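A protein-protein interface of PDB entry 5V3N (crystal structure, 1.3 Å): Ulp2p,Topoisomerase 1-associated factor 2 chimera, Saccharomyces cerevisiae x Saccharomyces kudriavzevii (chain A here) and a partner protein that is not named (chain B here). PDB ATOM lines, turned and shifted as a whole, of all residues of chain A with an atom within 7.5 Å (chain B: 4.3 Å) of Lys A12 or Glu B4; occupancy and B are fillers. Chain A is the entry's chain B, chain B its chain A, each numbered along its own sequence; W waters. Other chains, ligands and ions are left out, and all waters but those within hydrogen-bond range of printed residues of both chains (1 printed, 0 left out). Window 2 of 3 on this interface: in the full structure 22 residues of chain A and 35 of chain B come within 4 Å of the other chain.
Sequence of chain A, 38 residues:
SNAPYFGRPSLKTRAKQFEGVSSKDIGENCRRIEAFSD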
ATOM      1  N   PRO A   9     -16.981 -14.421 -22.882  1.00  0.00           N
ATOM      2  CA  PRO A   9     -17.938 -13.375 -22.536  1.00  0.00           C
ATOM      3  C   PRO A   9     -17.504 -12.591 -21.290  1.00  0.00           C
ATOM      4  O   PRO A   9     -16.745 -13.074 -20.438  1.00  0.00           O
ATOM      5  CB  PRO A   9     -19.248 -14.149 -22.330  1.00  0.00           C
ATOM      6  CG  PRO A   9     -18.853 -15.523 -22.063  1.00  0.00           C
ATOM      7  CD  PRO A   9     -17.522 -15.784 -22.648  1.00  0.00           C
ATOM      8  N   SER A  10     -17.944 -11.338 -21.217  1.00  0.00           N
ATOM      9  CA  SER A  10     -17.507 -10.454 -20.113  1.00  0.00           C
ATOM     10  C   SER A  10     -18.695  -9.659 -19.624  1.00  0.00           C
ATOM     11  O   SER A  10     -19.687  -9.489 -20.328  1.00  0.00           O
ATOM     12  CB  SER A  10     -16.373  -9.498 -20.474  1.00  0.00           C
ATOM     13  OG  SER A  10     -16.842  -8.218 -20.859  1.00  0.00           O
ATOM     14  N   LEU A  11     -18.615  -9.214 -18.373  1.00  0.00           N
ATOM     15  CA  LEU A  11     -19.677  -8.355 -17.894  1.00  0.00           C
ATOM     16  C   LEU A  11     -19.663  -6.982 -18.521  1.00  0.00           C
ATOM     17  O   LEU A  11     -20.645  -6.250 -18.366  1.00  0.00           O
ATOM     18  CB  LEU A  11     -19.570  -8.156 -16.384  1.00  0.00           C
ATOM     19  CG  LEU A  11     -19.813  -9.419 -15.506  1.00  0.00           C
ATOM     20  CD1 LEU A  11     -19.663  -9.031 -14.033  1.00  0.00           C
ATOM     21  CD2 LEU A  11     -21.164 -10.102 -15.787  1.00  0.00           C
ATOM     22  N   LYS A  12     -18.600  -6.650 -19.259  1.00  0.00           N
ATOM     23  CA  LYS A  12     -18.625  -5.332 -19.901  1.00  0.00           C
ATOM     24  C   LYS A  12     -19.826  -5.184 -20.826  1.00  0.00           C
ATOM     25  O   LYS A  12     -20.284  -4.065 -21.056  1.00  0.00           O
ATOM     26  CB  LYS A  12     -17.388  -5.059 -20.814  1.00  0.00           C
ATOM     27  CG  LYS A  12     -16.120  -4.642 -20.110  1.00  0.00           C
ATOM     28  CD  LYS A  12     -14.946  -4.413 -21.109  1.00  0.00           C
ATOM     29  CE  LYS A  12     -13.700  -3.763 -20.430  1.00  0.00           C
ATOM     30  NZ  LYS A  12     -12.762  -2.992 -21.354  1.00  0.00           N
ATOM     31  N   THR A  13     -20.264  -6.246 -21.483  1.00  0.00           N
ATOM     32  CA  THR A  13     -21.369  -6.121 -22.420  1.00  0.00           C
ATOM     33  C   THR A  13     -22.731  -5.971 -21.765  1.00  0.00           C
ATOM     34  O   THR A  13     -23.762  -5.896 -22.462  1.00  0.00           O
ATOM     35  CB  THR A  13     -21.367  -7.281 -23.396  1.00  0.00           C
ATOM     36  OG1 THR A  13     -21.504  -8.507 -22.675  1.00  0.00           O
ATOM     37  CG2 THR A  13     -20.056  -7.319 -24.159  1.00  0.00           C
ATOM     38  N   ARG A  14     -22.768  -5.922 -20.457  1.00  0.00           N
ATOM     39  CA  ARG A  14     -24.031  -5.752 -19.795  1.00  0.00           C
ATOM     40  C   ARG A  14     -24.418  -4.292 -19.697  1.00  0.00           C
ATOM     41  O   ARG A  14     -25.512  -3.958 -19.258  1.00  0.00           O
ATOM     42  CB  ARG A  14     -23.971  -6.316 -18.364  1.00  0.00           C
ATOM     43  CG  ARG A  14     -23.419  -7.718 -17.991  1.00  0.00           C
ATOM     44  CD  ARG A  14     -24.336  -8.702 -18.421  1.00  0.00           C
ATOM     45  NE  ARG A  14     -25.708  -8.671 -17.979  1.00  0.00           N
ATOM     46  CZ  ARG A  14     -26.627  -9.450 -18.545  1.00  0.00           C
ATOM     47  NH1 ARG A  14     -26.297 -10.217 -19.600  1.00  0.00           N
ATOM     48  NH2 ARG A  14     -27.883  -9.417 -18.141  1.00  0.00           N
ATOM     49  N   ALA A  15     -23.536  -3.374 -20.121  1.00  0.00           N
ATOM     50  CA  ALA A  15     -23.936  -1.972 -20.104  1.00  0.00           C
ATOM     51  C   ALA A  15     -25.258  -1.761 -20.836  1.00  0.00           C
ATOM     52  O   ALA A  15     -26.044  -0.898 -20.425  1.00  0.00           O
ATOM     53  CB  ALA A  15     -22.833  -1.097 -20.706  1.00  0.00           C
ATOM     54  N   LYS A  16     -25.497  -2.492 -21.952  1.00  0.00           N
ATOM     55  CA  LYS A  16     -26.726  -2.376 -22.727  1.00  0.00           C
ATOM     56  C   LYS A  16     -27.968  -2.607 -21.890  1.00  0.00           C
ATOM     57  O   LYS A  16     -29.052  -2.131 -22.248  1.00  0.00           O
ATOM     58  CB  LYS A  16     -26.749  -3.425 -23.843  1.00  0.00           C
ATOM     59  CG  LYS A  16     -28.030  -3.355 -24.710  1.00  0.00           C
ATOM     60  CD  LYS A  16     -28.196  -4.552 -25.677  1.00  0.00           C
ATOM     61  CE  LYS A  16     -29.445  -4.376 -26.584  1.00  0.00           C
ATOM     62  NZ  LYS A  16     -29.681  -5.468 -27.600  1.00  0.00           N
ATOM     63  N   ASN B   2      -4.779   2.162 -17.675  1.00  0.00           N
ATOM     64  CA  ASN B   2      -4.545   1.394 -16.431  1.00  0.00           C
ATOM     65  C   ASN B   2      -5.836   1.119 -15.670  1.00  0.00           C
ATOM     66  O   ASN B   2      -6.030   0.072 -15.033  1.00  0.00           O
ATOM     67  CB  ASN B   2      -3.607   2.194 -15.525  1.00  0.00           C
ATOM     68  N   SER B   3      -6.758   2.062 -15.760  1.00  0.00           N
ATOM     69  CA  SER B   3      -7.992   1.954 -15.006  1.00  0.00           C
ATOM     70  C   SER B   3      -8.857   0.822 -15.556  1.00  0.00           C
ATOM     71  O   SER B   3      -9.563   0.146 -14.794  1.00  0.00           O
ATOM     72  CB  SER B   3      -8.693   3.323 -14.978  1.00  0.00           C
ATOM     73  OG  SER B   3      -9.367   3.594 -16.173  1.00  0.00           O
ATOM     74  N   GLU B   4      -8.733   0.531 -16.851  1.00  0.00           N
ATOM     75  CA  GLU B   4      -9.524  -0.537 -17.451  1.00  0.00           C
ATOM     76  C   GLU B   4      -8.956  -1.925 -17.171  1.00  0.00           C
ATOM     77  O   GLU B   4      -9.737  -2.855 -16.945  1.00  0.00           O
ATOM     78  CB  GLU B   4      -9.626  -0.322 -18.948  1.00  0.00           C
ATOM     79  CG  GLU B   4     -10.522   0.884 -19.322  1.00  0.00           C
ATOM     80  CD  GLU B   4     -11.950   0.780 -18.767  1.00  0.00           C
ATOM     81  OE1 GLU B   4     -12.693  -0.142 -19.187  1.00  0.00           O
ATOM     82  OE2 GLU B   4     -12.351   1.640 -17.920  1.00  0.00           O
ATOM     83  N   VAL B   5      -7.638  -2.102 -17.143  1.00  0.00           N
ATOM     84  CA  VAL B   5      -7.038  -3.359 -16.671  1.00  0.00           C
ATOM     85  C   VAL B   5      -7.461  -3.629 -15.251  1.00  0.00           C
ATOM     86  O   VAL B   5      -7.814  -4.770 -14.860  1.00  0.00           O
ATOM     87  CB  VAL B   5      -5.491  -3.259 -16.799  1.00  0.00           C
ATOM     88  CG1 VAL B   5      -4.801  -4.476 -16.313  1.00  0.00           C
ATOM     89  CG2 VAL B   5      -5.106  -2.897 -18.194  1.00  0.00           C
ATOM     90  N   ILE B   6      -7.513  -2.585 -14.469  1.00  0.00           N
ATOM     91  CA  ILE B   6      -7.944  -2.768 -13.082  1.00  0.00           C
ATOM     92  C   ILE B   6      -9.433  -3.130 -13.005  1.00  0.00           C
ATOM     93  O   ILE B   6      -9.835  -3.996 -12.215  1.00  0.00           O
ATOM     94  CB  ILE B   6      -7.571  -1.505 -12.283  1.00  0.00           C
ATOM     95  CG1 ILE B   6      -6.046  -1.459 -12.137  1.00  0.00           C
ATOM     96  CG2 ILE B   6      -8.250  -1.420 -10.924  1.00  0.00           C
ATOM     97  CD1 ILE B   6      -5.537  -0.214 -11.458  1.00  0.00           C
ATOM     98  N   LYS B   7     -10.299  -2.452 -13.785  1.00  0.00           N
ATOM     99  CA  LYS B   7     -11.694  -2.873 -13.740  1.00  0.00           C
ATOM    100  C   LYS B   7     -11.847  -4.301 -14.208  1.00  0.00           C
ATOM    101  O   LYS B   7     -12.691  -5.028 -13.715  1.00  0.00           O
ATOM    102  CB  LYS B   7     -12.610  -1.964 -14.541  1.00  0.00           C
ATOM    103  CG  LYS B   7     -12.874  -0.651 -13.870  1.00  0.00           C
ATOM    104  CD  LYS B   7     -13.664   0.228 -14.833  1.00  0.00           C
ATOM    105  CE  LYS B   7     -15.127   0.184 -14.454  1.00  0.00           C
ATOM    106  NZ  LYS B   7     -16.022   1.112 -15.194  1.00  0.00           N
ATOM    107  N   ASP B   8     -11.060  -4.723 -15.175  1.00  0.00           N
ATOM    108  CA  ASP B   8     -11.147  -6.100 -15.591  1.00  0.00           C
ATOM    109  C   ASP B   8     -10.786  -7.006 -14.419  1.00  0.00           C
ATOM    110  O   ASP B   8     -11.394  -8.066 -14.232  1.00  0.00           O
ATOM    111  CB  ASP B   8     -10.198  -6.355 -16.764  1.00  0.00           C
ATOM    112  CG  ASP B   8     -10.712  -5.767 -18.058  1.00  0.00           C
ATOM    113  OD1 ASP B   8     -11.881  -5.324 -18.142  1.00  0.00           O
ATOM    114  OD2 ASP B   8      -9.959  -5.795 -19.029  1.00  0.00           O
ATOM    115  N   GLU B  11     -13.604  -7.453 -12.017  1.00  0.00           N
ATOM    116  CA  GLU B  11     -14.556  -8.406 -12.603  1.00  0.00           C
ATOM    117  C   GLU B  11     -14.173  -9.873 -12.334  1.00  0.00           C
ATOM    118  O   GLU B  11     -15.034 -10.681 -11.952  1.00  0.00           O
ATOM    119  CB  GLU B  11     -14.714  -8.111 -14.132  1.00  0.00           C
ATOM    120  CG  GLU B  11     -15.641  -9.153 -14.766  1.00  0.00           C
ATOM    121  CD  GLU B  11     -16.020  -8.867 -16.191  1.00  0.00           C
ATOM    122  OE1 GLU B  11     -16.485  -9.812 -16.857  1.00  0.00           O
ATOM    123  OE2 GLU B  11     -15.895  -7.691 -16.657  1.00  0.00           O
ATOM    124  N   ARG B  17     -18.958  -5.744 -11.991  1.00  0.00           N
ATOM    125  CA  ARG B  17     -18.459  -4.645 -12.815  1.00  0.00           C
ATOM    126  C   ARG B  17     -19.371  -3.459 -12.572  1.00  0.00           C
ATOM    127  O   ARG B  17     -20.604  -3.502 -12.693  1.00  0.00           O
ATOM    128  CB  ARG B  17     -18.450  -5.106 -14.261  1.00  0.00           C
ATOM    129  CG  ARG B  17     -17.968  -3.847 -15.176  1.00  0.00           C
ATOM    130  CD  ARG B  17     -17.753  -4.349 -16.469  1.00  0.00           C
ATOM    131  NE  ARG B  17     -16.539  -5.099 -16.523  1.00  0.00           N
ATOM    132  CZ  ARG B  17     -15.352  -4.594 -16.842  1.00  0.00           C
ATOM    133  NH1 ARG B  17     -15.195  -3.324 -17.002  1.00  0.00           N
ATOM    134  NH2 ARG B  17     -14.325  -5.368 -16.917  1.00  0.00           N
HETATM  135  O   HOH W   1     -12.487  -2.410 -18.211  1.00  0.00           O
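The side-chain carboxylate (OE1) of Glu B11 is in hydrogen-bond range of the backbone NH (N) of Leu A11 (2.7 Å).
The side-chain amino group (NZ) of Lys A12 is in salt-bridge range of the side-chain carboxylate (OE1) of Glu B4 (3.6 Å).
The backbone NH of Lys A12 is in hydrogen-bond range of the side-chain hydroxyl of Ser A10.
OE2 of Glu B11 lies within salt-bridge range of NE of Arg B17.
NH2 of Arg B17 is in salt-bridge range of OD1 of Asp B8.
OG1 of Thr A13 lies within hydrogen-bond range of O of Ser A10.
Among the printed residues, pairs that only touch across the chains: Lys A12 with Asp B8, Lys A12 with Arg B17, Ser A10 with Glu B11, Leu A11 with Arg B17 and Lys A12 with Glu B11.
Of chain B, only Glu B4 (3.6 Å), Asp B8 (3.3 Å), Glu B11 (3.9 Å) and Arg B17 (3.4 Å) come within 4 Å of Lys A12.
Glu B4 touches just one residue of chain A: Lys A12.
No residue of chain A comes within 4 Å of Ser B3.
Of the printed residues of chain A, Asp B8 touches Lys A12.
Of the printed residues of chain B, Ser A10 touches Glu B11 (3.5 Å).
Of the printed residues of chain B, Leu A11 touches Glu B11 and Arg B17.
Printed residues of chain A within 4 Å of Glu B11: Ser A10, Leu A11 and Lys A12.
Printed residues of chain A within 4 Å of Arg B17: Leu A11 and Lys A12.
Arg A14 touches none of the printed residues of chain B.
Pro A9 touches none of the printed residues of chain B.
The nearest printed residue of chain B that does not touch Lys A12 is Lys B7 (6.3 Å).
The nearest printed residue of chain A that does not touch Glu B4 is Ser A10 (9.2 Å).
Of the 9 printed residues of chain B, 4 touch a printed residue of chain A.
Water W1 lies within hydrogen-bond range of OE1 of Glu B4, OD1 of Asp B8, NH1 of Arg B17 and NZ of Lys A12.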
